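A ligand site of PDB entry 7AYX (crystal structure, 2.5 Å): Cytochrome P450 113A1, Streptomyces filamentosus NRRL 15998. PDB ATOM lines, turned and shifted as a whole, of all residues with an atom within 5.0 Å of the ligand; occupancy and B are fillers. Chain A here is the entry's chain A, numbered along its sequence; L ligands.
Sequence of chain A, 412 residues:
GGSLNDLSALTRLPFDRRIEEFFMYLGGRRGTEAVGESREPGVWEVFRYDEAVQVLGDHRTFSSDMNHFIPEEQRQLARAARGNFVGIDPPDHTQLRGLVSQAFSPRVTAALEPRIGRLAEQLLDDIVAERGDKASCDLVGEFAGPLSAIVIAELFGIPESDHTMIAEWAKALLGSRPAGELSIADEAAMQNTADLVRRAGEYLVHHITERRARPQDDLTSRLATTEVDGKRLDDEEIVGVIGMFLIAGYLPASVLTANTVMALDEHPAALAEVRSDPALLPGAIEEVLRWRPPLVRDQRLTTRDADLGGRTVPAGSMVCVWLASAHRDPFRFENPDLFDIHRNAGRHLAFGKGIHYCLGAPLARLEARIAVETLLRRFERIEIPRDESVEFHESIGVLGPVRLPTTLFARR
SG of Cys 358 binds FE1 of the ligand, 2.4 Å away. O4 of the ligand is in salt-bridge range of NH1 of Arg 97 (2.6 Å). An oxygen (O1) of the ligand lies within salt-bridge range of the guanidinium group (NH2) of Arg 300, 2.9 Å away. An oxygen (O1) of the ligand sits close to the side-chain carboxylate (OD2) of Asp 298 (2.9 Å). NE2 of His 93 is in hydrogen-bond range of O4 of the ligand (2.8 Å).
Phe 85 touches the ligand. Val 86 touches the ligand. CG1 of Ile 152 touches C26 of the ligand (3.8 Å). O of Phe 245 touches C26 of the ligand (3.3 Å). Ala 248 touches the ligand (CB to C27, 3.9 Å). CA of Gly 249 touches C21 of the ligand, 3.4 Å away. Pro 252 touches the ligand (CB to C15, 3.3 Å). Ala 253 touches the ligand (N to C18, 3.4 Å). Leu 256 touches the ligand (CD2 to C19, 3.4 Å). Leu 295 touches the ligand. Ala 350 touches the ligand. Phe 351 touches the ligand. Gly 352 touches the ligand. O of Ile 355 touches O4 of the ligand (3.6 Å). His 356 touches the ligand (CD2 to O3, 3.0 Å). O of Tyr 357 touches C33 of the ligand, 3.9 Å away. Gly 360 touches the ligand. Ala 364 touches the ligand. Hydrophobic or aromatic side chains within 4 Å of the ligand: Phe 85, Val 86, His 93, Ile 152, Phe 245, Ala 248, Pro 252, Leu 256, Leu 295, Phe 351, His 356 and Ala 364.
O of Phe 85 is in hydrogen-bond range of NE2 of His 356, 3.4 Å away. The side-chain sulfur of Met 244 sits at hydrogen-bond distance from the backbone NH of Phe 85. The side-chain hydroxyl (OG) of Ser 64 lies close to a ring nitrogen (ND1) of His 356, at 3.3 Å. The backbone carbonyl oxygen of Phe 351 is in hydrogen-bond range of the backbone NH of Cys 358 (2.9 Å). SG of Cys 358 lies close to N of Gly 360 (3.2 Å). N of Ala 361 sits close to SG of Cys 358. NE2 of His 356 lies within hydrogen-bond range of O of Val 86. NH1 of Arg 97 lies within hydrogen-bond range of O of Ile 355.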
ATOM      1  N   LEU A  56     -12.721  -4.927  -4.177  1.00  0.00           N
ATOM      2  CA  LEU A  56     -13.798  -5.698  -3.551  1.00  0.00           C
ATOM      3  C   LEU A  56     -13.977  -7.060  -4.230  1.00  0.00           C
ATOM      4  O   LEU A  56     -14.266  -8.058  -3.575  1.00  0.00           O
ATOM      5  CB  LEU A  56     -15.102  -4.924  -3.589  1.00  0.00           C
ATOM      6  CG  LEU A  56     -15.061  -3.559  -2.902  1.00  0.00           C
ATOM      7  CD1 LEU A  56     -16.343  -2.802  -3.172  1.00  0.00           C
ATOM      8  CD2 LEU A  56     -14.803  -3.708  -1.412  1.00  0.00           C
ATOM      9  N   SER A  64     -10.504  -9.726   3.820  1.00  0.00           N
ATOM     10  CA  SER A  64     -11.411  -9.128   4.809  1.00  0.00           C
ATOM     11  C   SER A  64     -11.005  -9.537   6.234  1.00  0.00           C
ATOM     12  O   SER A  64     -11.495  -8.976   7.222  1.00  0.00           O
ATOM     13  CB  SER A  64     -12.860  -9.558   4.529  1.00  0.00           C
ATOM     14  OG  SER A  64     -13.237  -9.267   3.199  1.00  0.00           O
ATOM     15  N   PHE A  85     -19.152 -13.970   9.780  1.00  0.00           N
ATOM     16  CA  PHE A  85     -18.435 -14.217   8.539  1.00  0.00           C
ATOM     17  C   PHE A  85     -18.077 -12.942   7.762  1.00  0.00           C
ATOM     18  O   PHE A  85     -17.575 -13.024   6.645  1.00  0.00           O
ATOM     19  CB  PHE A  85     -19.186 -15.212   7.635  1.00  0.00           C
ATOM     20  CG  PHE A  85     -20.609 -14.836   7.318  1.00  0.00           C
ATOM     21  CD1 PHE A  85     -20.903 -13.786   6.451  1.00  0.00           C
ATOM     22  CD2 PHE A  85     -21.664 -15.562   7.858  1.00  0.00           C
ATOM     23  CE1 PHE A  85     -22.214 -13.472   6.145  1.00  0.00           C
ATOM     24  CE2 PHE A  85     -22.975 -15.248   7.552  1.00  0.00           C
ATOM     25  CZ  PHE A  85     -23.250 -14.203   6.696  1.00  0.00           C
ATOM     26  N   VAL A  86     -18.311 -11.780   8.374  1.00  0.00           N
ATOM     27  CA  VAL A  86     -17.986 -10.493   7.742  1.00  0.00           C
ATOM     28  C   VAL A  86     -16.469 -10.272   7.692  1.00  0.00           C
ATOM     29  O   VAL A  86     -15.961  -9.651   6.742  1.00  0.00           O
ATOM     30  CB  VAL A  86     -18.725  -9.286   8.388  1.00  0.00           C
ATOM     31  CG1 VAL A  86     -18.150  -8.949   9.755  1.00  0.00           C
ATOM     32  CG2 VAL A  86     -18.679  -8.075   7.454  1.00  0.00           C
ATOM     33  N   HIS A  93     -16.111 -18.409   4.684  1.00  0.00           N
ATOM     34  CA  HIS A  93     -17.248 -17.487   4.421  1.00  0.00           C
ATOM     35  C   HIS A  93     -18.306 -18.157   3.569  1.00  0.00           C
ATOM     36  O   HIS A  93     -19.486 -18.028   3.901  1.00  0.00           O
ATOM     37  CB  HIS A  93     -16.697 -16.245   3.712  1.00  0.00           C
ATOM     38  CG  HIS A  93     -17.714 -15.239   3.316  1.00  0.00           C
ATOM     39  ND1 HIS A  93     -18.135 -15.090   2.025  1.00  0.00           N
ATOM     40  CD2 HIS A  93     -18.377 -14.314   4.045  1.00  0.00           C
ATOM     41  CE1 HIS A  93     -19.020 -14.122   1.964  1.00  0.00           C
ATOM     42  NE2 HIS A  93     -19.190 -13.636   3.186  1.00  0.00           N
ATOM     43  N   ARG A  97     -22.152 -18.191   4.955  1.00  0.00           N
ATOM     44  CA  ARG A  97     -23.037 -17.290   4.239  1.00  0.00           C
ATOM     45  C   ARG A  97     -24.066 -18.088   3.436  1.00  0.00           C
ATOM     46  O   ARG A  97     -25.211 -17.677   3.317  1.00  0.00           O
ATOM     47  CB  ARG A  97     -22.250 -16.356   3.315  1.00  0.00           C
ATOM     48  CG  ARG A  97     -23.077 -15.215   2.747  1.00  0.00           C
ATOM     49  CD  ARG A  97     -22.336 -14.435   1.663  1.00  0.00           C
ATOM     50  NE  ARG A  97     -23.258 -13.748   0.766  1.00  0.00           N
ATOM     51  CZ  ARG A  97     -23.606 -12.456   0.829  1.00  0.00           C
ATOM     52  NH1 ARG A  97     -23.104 -11.647   1.762  1.00  0.00           N
ATOM     53  NH2 ARG A  97     -24.458 -11.970  -0.053  1.00  0.00           N
ATOM     54  N   ILE A 152     -34.861  -5.129  12.808  1.00  0.00           N
ATOM     55  CA  ILE A 152     -33.942  -6.266  12.901  1.00  0.00           C
ATOM     56  C   ILE A 152     -34.428  -7.248  13.981  1.00  0.00           C
ATOM     57  O   ILE A 152     -34.308  -8.472  13.818  1.00  0.00           O
ATOM     58  CB  ILE A 152     -32.466  -5.854  13.130  1.00  0.00           C
ATOM     59  CG1 ILE A 152     -31.949  -4.998  11.969  1.00  0.00           C
ATOM     60  CG2 ILE A 152     -31.579  -7.089  13.264  1.00  0.00           C
ATOM     61  CD1 ILE A 152     -30.656  -4.268  12.271  1.00  0.00           C
ATOM     62  N   LEU A 155     -37.377  -9.205  12.395  1.00  0.00           N
ATOM     63  CA  LEU A 155     -36.826 -10.208  11.479  1.00  0.00           C
ATOM     64  C   LEU A 155     -36.537 -11.532  12.193  1.00  0.00           C
ATOM     65  O   LEU A 155     -36.866 -12.605  11.687  1.00  0.00           O
ATOM     66  CB  LEU A 155     -35.546  -9.671  10.832  1.00  0.00           C
ATOM     67  CG  LEU A 155     -34.709 -10.660  10.005  1.00  0.00           C
ATOM     68  CD1 LEU A 155     -35.527 -11.253   8.862  1.00  0.00           C
ATOM     69  CD2 LEU A 155     -33.448  -9.986   9.477  1.00  0.00           C
ATOM     70  N   MET A 244     -24.213 -10.403  14.471  1.00  0.00           N
ATOM     71  CA  MET A 244     -23.587  -9.794  13.303  1.00  0.00           C
ATOM     72  C   MET A 244     -24.580  -8.911  12.536  1.00  0.00           C
ATOM     73  O   MET A 244     -24.208  -7.835  12.064  1.00  0.00           O
ATOM     74  CB  MET A 244     -23.011 -10.871  12.368  1.00  0.00           C
ATOM     75  CG  MET A 244     -22.617 -10.376  10.973  1.00  0.00           C
ATOM     76  SD  MET A 244     -21.986 -11.674   9.897  1.00  0.00           S
ATOM     77  CE  MET A 244     -23.461 -12.683   9.669  1.00  0.00           C
ATOM     78  N   PHE A 245     -25.817  -9.388  12.399  1.00  0.00           N
ATOM     79  CA  PHE A 245     -26.893  -8.660  11.738  1.00  0.00           C
ATOM     80  C   PHE A 245     -27.198  -7.340  12.458  1.00  0.00           C
ATOM     81  O   PHE A 245     -27.331  -6.301  11.812  1.00  0.00           O
ATOM     82  CB  PHE A 245     -28.164  -9.505  11.656  1.00  0.00           C
ATOM     83  CG  PHE A 245     -28.282 -10.323  10.398  1.00  0.00           C
ATOM     84  CD1 PHE A 245     -27.284 -11.202  10.023  1.00  0.00           C
ATOM     85  CD2 PHE A 245     -29.430 -10.244   9.610  1.00  0.00           C
ATOM     86  CE1 PHE A 245     -27.407 -11.975   8.878  1.00  0.00           C
ATOM     87  CE2 PHE A 245     -29.556 -11.001   8.468  1.00  0.00           C
ATOM     88  CZ  PHE A 245     -28.546 -11.878   8.100  1.00  0.00           C
ATOM     89  N   LEU A 246     -27.313  -7.403  13.788  1.00  0.00           N
ATOM     90  CA  LEU A 246     -27.584  -6.205  14.594  1.00  0.00           C
ATOM     91  C   LEU A 246     -26.461  -5.174  14.470  1.00  0.00           C
ATOM     92  O   LEU A 246     -26.736  -3.985  14.300  1.00  0.00           O
ATOM     93  CB  LEU A 246     -27.773  -6.598  16.062  1.00  0.00           C
ATOM     94  CG  LEU A 246     -29.089  -7.301  16.357  1.00  0.00           C
ATOM     95  CD1 LEU A 246     -28.958  -8.256  17.532  1.00  0.00           C
ATOM     96  CD2 LEU A 246     -30.202  -6.286  16.585  1.00  0.00           C
ATOM     97  N   ALA A 248     -23.905  -4.970  12.163  1.00  0.00           N
ATOM     98  CA  ALA A 248     -23.727  -4.513  10.797  1.00  0.00           C
ATOM     99  C   ALA A 248     -24.882  -3.630  10.324  1.00  0.00           C
ATOM    100  O   ALA A 248     -24.669  -2.684   9.563  1.00  0.00           O
ATOM    101  CB  ALA A 248     -23.577  -5.708   9.866  1.00  0.00           C
ATOM    102  N   GLY A 249     -26.099  -3.942  10.781  1.00  0.00           N
ATOM    103  CA  GLY A 249     -27.328  -3.399  10.212  1.00  0.00           C
ATOM    104  C   GLY A 249     -27.962  -2.177  10.850  1.00  0.00           C
ATOM    105  O   GLY A 249     -28.641  -1.426  10.168  1.00  0.00           O
ATOM    106  N   PRO A 252     -26.191   1.902  10.016  1.00  0.00           N
ATOM    107  CA  PRO A 252     -26.342   2.268   8.613  1.00  0.00           C
ATOM    108  C   PRO A 252     -27.793   2.468   8.167  1.00  0.00           C
ATOM    109  O   PRO A 252     -28.078   3.434   7.476  1.00  0.00           O
ATOM    110  CB  PRO A 252     -25.723   1.087   7.869  1.00  0.00           C
ATOM    111  CG  PRO A 252     -24.753   0.510   8.836  1.00  0.00           C
ATOM    112  CD  PRO A 252     -25.400   0.668  10.182  1.00  0.00           C
ATOM    113  N   ALA A 253     -28.686   1.549   8.552  1.00  0.00           N
ATOM    114  CA  ALA A 253     -30.100   1.637   8.201  1.00  0.00           C
ATOM    115  C   ALA A 253     -30.746   2.922   8.738  1.00  0.00           C
ATOM    116  O   ALA A 253     -31.493   3.579   8.005  1.00  0.00           O
ATOM    117  CB  ALA A 253     -30.854   0.428   8.706  1.00  0.00           C
ATOM    118  N   LEU A 256     -29.312   5.758   6.765  1.00  0.00           N
ATOM    119  CA  LEU A 256     -29.934   5.825   5.418  1.00  0.00           C
ATOM    120  C   LEU A 256     -31.270   6.555   5.533  1.00  0.00           C
ATOM    121  O   LEU A 256     -31.525   7.455   4.716  1.00  0.00           O
ATOM    122  CB  LEU A 256     -30.126   4.403   4.873  1.00  0.00           C
ATOM    123  CG  LEU A 256     -30.830   4.301   3.519  1.00  0.00           C
ATOM    124  CD1 LEU A 256     -30.176   5.194   2.490  1.00  0.00           C
ATOM    125  CD2 LEU A 256     -30.869   2.856   3.040  1.00  0.00           C
ATOM    126  N   LEU A 289     -27.929   6.734  -1.356  1.00  0.00           N
ATOM    127  CA  LEU A 289     -26.880   5.725  -1.168  1.00  0.00           C
ATOM    128  C   LEU A 289     -25.594   6.016  -1.950  1.00  0.00           C
ATOM    129  O   LEU A 289     -24.513   5.660  -1.492  1.00  0.00           O
ATOM    130  CB  LEU A 289     -27.392   4.340  -1.541  1.00  0.00           C
ATOM    131  CG  LEU A 289     -28.399   3.756  -0.539  1.00  0.00           C
ATOM    132  CD1 LEU A 289     -29.266   2.702  -1.211  1.00  0.00           C
ATOM    133  CD2 LEU A 289     -27.684   3.177   0.672  1.00  0.00           C
ATOM    134  N   PRO A 294     -24.333   6.090   3.916  1.00  0.00           N
ATOM    135  CA  PRO A 294     -24.115   5.902   5.351  1.00  0.00           C
ATOM    136  C   PRO A 294     -22.713   5.394   5.692  1.00  0.00           C
ATOM    137  O   PRO A 294     -22.019   6.033   6.502  1.00  0.00           O
ATOM    138  CB  PRO A 294     -25.183   4.871   5.731  1.00  0.00           C
ATOM    139  CG  PRO A 294     -26.272   5.059   4.720  1.00  0.00           C
ATOM    140  CD  PRO A 294     -25.589   5.482   3.447  1.00  0.00           C
ATOM    141  N   LEU A 295     -22.304   4.277   5.086  1.00  0.00           N
ATOM    142  CA  LEU A 295     -20.951   3.771   5.221  1.00  0.00           C
ATOM    143  C   LEU A 295     -20.161   4.276   4.035  1.00  0.00           C
ATOM    144  O   LEU A 295     -20.511   4.006   2.884  1.00  0.00           O
ATOM    145  CB  LEU A 295     -20.925   2.253   5.279  1.00  0.00           C
ATOM    146  CG  LEU A 295     -21.688   1.632   6.437  1.00  0.00           C
ATOM    147  CD1 LEU A 295     -21.357   0.146   6.530  1.00  0.00           C
ATOM    148  CD2 LEU A 295     -21.382   2.326   7.758  1.00  0.00           C
ATOM    149  N   ASP A 298     -14.731   1.063   3.035  1.00  0.00           N
ATOM    150  CA  ASP A 298     -14.750  -0.388   3.200  1.00  0.00           C
ATOM    151  C   ASP A 298     -13.284  -0.785   3.166  1.00  0.00           C
ATOM    152  O   ASP A 298     -12.553  -0.358   2.274  1.00  0.00           O
ATOM    153  CB  ASP A 298     -15.539  -1.031   2.042  1.00  0.00           C
ATOM    154  CG  ASP A 298     -16.076  -2.428   2.374  1.00  0.00           C
ATOM    155  OD1 ASP A 298     -15.846  -2.938   3.490  1.00  0.00           O
ATOM    156  OD2 ASP A 298     -16.737  -3.005   1.487  1.00  0.00           O
ATOM    157  N   ARG A 300      -9.862  -3.430   3.442  1.00  0.00           N
ATOM    158  CA  ARG A 300      -9.272  -4.718   3.114  1.00  0.00           C
ATOM    159  C   ARG A 300      -7.781  -4.731   3.503  1.00  0.00           C
ATOM    160  O   ARG A 300      -7.212  -3.693   3.853  1.00  0.00           O
ATOM    161  CB  ARG A 300      -9.422  -5.017   1.617  1.00  0.00           C
ATOM    162  CG  ARG A 300     -10.864  -5.172   1.135  1.00  0.00           C
ATOM    163  CD  ARG A 300     -11.487  -6.447   1.663  1.00  0.00           C
ATOM    164  NE  ARG A 300     -12.818  -6.722   1.129  1.00  0.00           N
ATOM    165  CZ  ARG A 300     -13.945  -6.150   1.545  1.00  0.00           C
ATOM    166  NH1 ARG A 300     -13.950  -5.239   2.501  1.00  0.00           N
ATOM    167  NH2 ARG A 300     -15.101  -6.498   0.977  1.00  0.00           N
ATOM    168  N   LEU A 323     -15.654   4.396  -0.848  1.00  0.00           N
ATOM    169  CA  LEU A 323     -16.907   4.211  -1.574  1.00  0.00           C
ATOM    170  C   LEU A 323     -17.491   5.583  -1.964  1.00  0.00           C
ATOM    171  O   LEU A 323     -17.984   5.761  -3.067  1.00  0.00           O
ATOM    172  CB  LEU A 323     -17.921   3.436  -0.722  1.00  0.00           C
ATOM    173  CG  LEU A 323     -17.484   2.078  -0.155  1.00  0.00           C
ATOM    174  CD1 LEU A 323     -18.565   1.519   0.751  1.00  0.00           C
ATOM    175  CD2 LEU A 323     -17.149   1.091  -1.264  1.00  0.00           C
ATOM    176  N   LEU A 349     -21.847   1.452  -4.883  1.00  0.00           N
ATOM    177  CA  LEU A 349     -21.213   0.437  -4.035  1.00  0.00           C
ATOM    178  C   LEU A 349     -21.560   0.561  -2.539  1.00  0.00           C
ATOM    179  O   LEU A 349     -20.878  -0.010  -1.694  1.00  0.00           O
ATOM    180  CB  LEU A 349     -19.698   0.523  -4.180  1.00  0.00           C
ATOM    181  CG  LEU A 349     -19.111   0.482  -5.588  1.00  0.00           C
ATOM    182  CD1 LEU A 349     -17.620   0.779  -5.524  1.00  0.00           C
ATOM    183  CD2 LEU A 349     -19.351  -0.870  -6.244  1.00  0.00           C
ATOM    184  N   ALA A 350     -22.617   1.312  -2.222  1.00  0.00           N
ATOM    185  CA  ALA A 350     -23.052   1.570  -0.834  1.00  0.00           C
ATOM    186  C   ALA A 350     -23.266   0.321  -0.001  1.00  0.00           C
ATOM    187  O   ALA A 350     -23.055   0.343   1.212  1.00  0.00           O
ATOM    188  CB  ALA A 350     -24.318   2.426  -0.822  1.00  0.00           C
ATOM    189  N   PHE A 351     -23.709  -0.766  -0.658  1.00  0.00           N
ATOM    190  CA  PHE A 351     -23.933  -2.074  -0.048  1.00  0.00           C
ATOM    191  C   PHE A 351     -22.800  -3.045  -0.340  1.00  0.00           C
ATOM    192  O   PHE A 351     -22.925  -4.247  -0.095  1.00  0.00           O
ATOM    193  CB  PHE A 351     -25.257  -2.669  -0.558  1.00  0.00           C
ATOM    194  CG  PHE A 351     -26.483  -1.936  -0.074  1.00  0.00           C
ATOM    195  CD1 PHE A 351     -26.762  -1.841   1.277  1.00  0.00           C
ATOM    196  CD2 PHE A 351     -27.378  -1.381  -0.981  1.00  0.00           C
ATOM    197  CE1 PHE A 351     -27.887  -1.182   1.734  1.00  0.00           C
ATOM    198  CE2 PHE A 351     -28.511  -0.726  -0.539  1.00  0.00           C
ATOM    199  CZ  PHE A 351     -28.771  -0.622   0.820  1.00  0.00           C
ATOM    200  N   GLY A 352     -21.694  -2.514  -0.877  1.00  0.00           N
ATOM    201  CA  GLY A 352     -20.518  -3.287  -1.218  1.00  0.00           C
ATOM    202  C   GLY A 352     -20.621  -3.944  -2.573  1.00  0.00           C
ATOM    203  O   GLY A 352     -21.423  -3.549  -3.408  1.00  0.00           O
ATOM    204  N   ILE A 355     -18.530 -11.061  -2.896  1.00  0.00           N
ATOM    205  CA  ILE A 355     -18.988 -12.103  -1.971  1.00  0.00           C
ATOM    206  C   ILE A 355     -19.576 -11.604  -0.644  1.00  0.00           C
ATOM    207  O   ILE A 355     -20.432 -12.272  -0.055  1.00  0.00           O
ATOM    208  CB  ILE A 355     -17.869 -13.120  -1.683  1.00  0.00           C
ATOM    209  CG1 ILE A 355     -16.696 -12.460  -0.932  1.00  0.00           C
ATOM    210  CG2 ILE A 355     -17.383 -13.760  -2.978  1.00  0.00           C
ATOM    211  CD1 ILE A 355     -15.629 -13.437  -0.484  1.00  0.00           C
ATOM    212  N   HIS A 356     -19.103 -10.439  -0.177  1.00  0.00           N
ATOM    213  CA  HIS A 356     -19.529  -9.824   1.100  1.00  0.00           C
ATOM    214  C   HIS A 356     -20.680  -8.821   0.943  1.00  0.00           C
ATOM    215  O   HIS A 356     -21.026  -8.129   1.901  1.00  0.00           O
ATOM    216  CB  HIS A 356     -18.353  -9.134   1.806  1.00  0.00           C
ATOM    217  CG  HIS A 356     -17.421 -10.074   2.501  1.00  0.00           C
ATOM    218  ND1 HIS A 356     -16.158 -10.367   2.023  1.00  0.00           N
ATOM    219  CD2 HIS A 356     -17.557 -10.784   3.648  1.00  0.00           C
ATOM    220  CE1 HIS A 356     -15.568 -11.230   2.829  1.00  0.00           C
ATOM    221  NE2 HIS A 356     -16.393 -11.491   3.824  1.00  0.00           N
ATOM    222  N   TYR A 357     -21.271  -8.745  -0.259  1.00  0.00           N
ATOM    223  CA  TYR A 357     -22.402  -7.853  -0.544  1.00  0.00           C
ATOM    224  C   TYR A 357     -23.462  -7.955   0.554  1.00  0.00           C
ATOM    225  O   TYR A 357     -23.809  -9.050   0.998  1.00  0.00           O
ATOM    226  CB  TYR A 357     -23.033  -8.169  -1.901  1.00  0.00           C
ATOM    227  CG  TYR A 357     -24.111  -7.172  -2.314  1.00  0.00           C
ATOM    228  CD1 TYR A 357     -23.778  -5.995  -2.986  1.00  0.00           C
ATOM    229  CD2 TYR A 357     -25.451  -7.395  -2.014  1.00  0.00           C
ATOM    230  CE1 TYR A 357     -24.748  -5.088  -3.357  1.00  0.00           C
ATOM    231  CE2 TYR A 357     -26.421  -6.488  -2.385  1.00  0.00           C
ATOM    232  CZ  TYR A 357     -26.072  -5.326  -3.054  1.00  0.00           C
ATOM    233  OH  TYR A 357     -27.035  -4.411  -3.424  1.00  0.00           O
ATOM    234  N   CYS A 358     -23.969  -6.781   0.979  1.00  0.00           N
ATOM    235  CA  CYS A 358     -24.856  -6.667   2.129  1.00  0.00           C
ATOM    236  C   CYS A 358     -26.073  -7.584   2.017  1.00  0.00           C
ATOM    237  O   CYS A 358     -26.856  -7.463   1.077  1.00  0.00           O
ATOM    238  CB  CYS A 358     -25.336  -5.226   2.282  1.00  0.00           C
ATOM    239  SG  CYS A 358     -26.442  -5.003   3.703  1.00  0.00           S
ATOM    240  N   LEU A 359     -26.216  -8.495   2.982  1.00  0.00           N
ATOM    241  CA  LEU A 359     -27.378  -9.377   3.055  1.00  0.00           C
ATOM    242  C   LEU A 359     -28.643  -8.615   3.483  1.00  0.00           C
ATOM    243  O   LEU A 359     -29.751  -9.074   3.243  1.00  0.00           O
ATOM    244  CB  LEU A 359     -27.125 -10.537   4.012  1.00  0.00           C
ATOM    245  CG  LEU A 359     -26.209 -11.647   3.486  1.00  0.00           C
ATOM    246  CD1 LEU A 359     -25.770 -12.564   4.623  1.00  0.00           C
ATOM    247  CD2 LEU A 359     -26.896 -12.474   2.401  1.00  0.00           C
ATOM    248  N   GLY A 360     -28.460  -7.438   4.100  1.00  0.00           N
ATOM    249  CA  GLY A 360     -29.571  -6.630   4.558  1.00  0.00           C
ATOM    250  C   GLY A 360     -30.043  -5.556   3.597  1.00  0.00           C
ATOM    251  O   GLY A 360     -30.943  -4.775   3.941  1.00  0.00           O
ATOM    252  N   ALA A 361     -29.443  -5.502   2.412  1.00  0.00           N
ATOM    253  CA  ALA A 361     -29.710  -4.448   1.426  1.00  0.00           C
ATOM    254  C   ALA A 361     -31.193  -4.354   1.083  1.00  0.00           C
ATOM    255  O   ALA A 361     -31.767  -3.276   1.138  1.00  0.00           O
ATOM    256  CB  ALA A 361     -28.847  -4.623   0.179  1.00  0.00           C
ATOM    257  N   LEU A 363     -33.791  -5.344   2.852  1.00  0.00           N
ATOM    258  CA  LEU A 363     -34.495  -4.915   4.059  1.00  0.00           C
ATOM    259  C   LEU A 363     -34.293  -3.416   4.343  1.00  0.00           C
ATOM    260  O   LEU A 363     -35.231  -2.742   4.740  1.00  0.00           O
ATOM    261  CB  LEU A 363     -34.062  -5.755   5.271  1.00  0.00           C
ATOM    262  CG  LEU A 363     -34.783  -5.474   6.592  1.00  0.00           C
ATOM    263  CD1 LEU A 363     -36.297  -5.577   6.435  1.00  0.00           C
ATOM    264  CD2 LEU A 363     -34.298  -6.437   7.663  1.00  0.00           C
ATOM    265  N   ALA A 364     -33.062  -2.931   4.140  1.00  0.00           N
ATOM    266  CA  ALA A 364     -32.720  -1.523   4.355  1.00  0.00           C
ATOM    267  C   ALA A 364     -33.474  -0.602   3.404  1.00  0.00           C
ATOM    268  O   ALA A 364     -33.912   0.472   3.808  1.00  0.00           O
ATOM    269  CB  ALA A 364     -31.216  -1.318   4.208  1.00  0.00           C
HETATM  270  C1  LIG L   1     -22.343  -6.287   4.760  1.00  0.00           C
HETATM  271  C2  LIG L   1     -23.629  -1.690   4.086  1.00  0.00           C
HETATM  272  C3  LIG L   1     -27.850  -2.551   6.341  1.00  0.00           C
HETATM  273  C4  LIG L   1     -26.403  -7.057   7.295  1.00  0.00           C
HETATM  274  C5  LIG L   1     -22.368  -4.982   4.350  1.00  0.00           C
HETATM  275  C6  LIG L   1     -21.380  -4.367   3.553  1.00  0.00           C
HETATM  276  C7  LIG L   1     -21.747  -3.080   3.370  1.00  0.00           C
HETATM  277  C8  LIG L   1     -22.952  -2.878   4.055  1.00  0.00           C
HETATM  278  C9  LIG L   1     -20.992  -2.040   2.581  1.00  0.00           C
HETATM  279  C10 LIG L   1     -20.145  -5.000   2.967  1.00  0.00           C
HETATM  280  C11 LIG L   1     -19.011  -5.067   3.970  1.00  0.00           C
HETATM  281  C12 LIG L   1     -17.807  -5.691   3.317  1.00  0.00           C
HETATM  282  O1  LIG L   1     -17.711  -5.703   2.075  1.00  0.00           O
HETATM  283  O2  LIG L   1     -16.911  -6.193   4.002  1.00  0.00           O
HETATM  284  C13 LIG L   1     -24.892  -1.570   4.650  1.00  0.00           C
HETATM  285  C14 LIG L   1     -25.599  -0.359   4.609  1.00  0.00           C
HETATM  286  C15 LIG L   1     -26.795  -0.576   5.223  1.00  0.00           C
HETATM  287  C16 LIG L   1     -26.774  -1.975   5.665  1.00  0.00           C
HETATM  288  C17 LIG L   1     -25.100   0.919   3.978  1.00  0.00           C
HETATM  289  C18 LIG L   1     -27.902   0.350   5.474  1.00  0.00           C
HETATM  290  C19 LIG L   1     -28.394   1.103   4.511  1.00  0.00           C
HETATM  291  C20 LIG L   1     -27.838  -3.860   6.781  1.00  0.00           C
HETATM  292  C21 LIG L   1     -28.906  -4.516   7.396  1.00  0.00           C
HETATM  293  C22 LIG L   1     -28.480  -5.799   7.668  1.00  0.00           C
HETATM  294  C23 LIG L   1     -27.154  -5.922   7.199  1.00  0.00           C
HETATM  295  C24 LIG L   1     -30.246  -3.901   7.705  1.00  0.00           C
HETATM  296  C25 LIG L   1     -29.258  -6.868   8.300  1.00  0.00           C
HETATM  297  C26 LIG L   1     -29.671  -6.761   9.552  1.00  0.00           C
HETATM  298  C27 LIG L   1     -25.170  -7.155   6.659  1.00  0.00           C
HETATM  299  C28 LIG L   1     -24.431  -8.409   6.709  1.00  0.00           C
HETATM  300  C29 LIG L   1     -23.317  -8.188   6.002  1.00  0.00           C
HETATM  301  C30 LIG L   1     -23.373  -6.807   5.524  1.00  0.00           C
HETATM  302  C31 LIG L   1     -24.828  -9.679   7.404  1.00  0.00           C
HETATM  303  C32 LIG L   1     -22.200  -9.150   5.757  1.00  0.00           C
HETATM  304  C33 LIG L   1     -22.451 -10.001   4.535  1.00  0.00           C
HETATM  305  C34 LIG L   1     -21.154 -10.710   4.319  1.00  0.00           C
HETATM  306  O3  LIG L   1     -20.184 -10.446   5.055  1.00  0.00           O
HETATM  307  O4  LIG L   1     -21.048 -11.543   3.413  1.00  0.00           O
HETATM  308  N1  LIG L   1     -23.328  -4.047   4.653  1.00  0.00           N
HETATM  309  N2  LIG L   1     -25.610  -2.502   5.277  1.00  0.00           N
HETATM  310  N3  LIG L   1     -26.790  -4.723   6.666  1.00  0.00           N
HETATM  311  N4  LIG L   1     -24.498  -6.239   5.953  1.00  0.00           N
HETATM  312 FE1  LIG L   1     -25.025  -4.488   5.590  1.00  0.00          FE
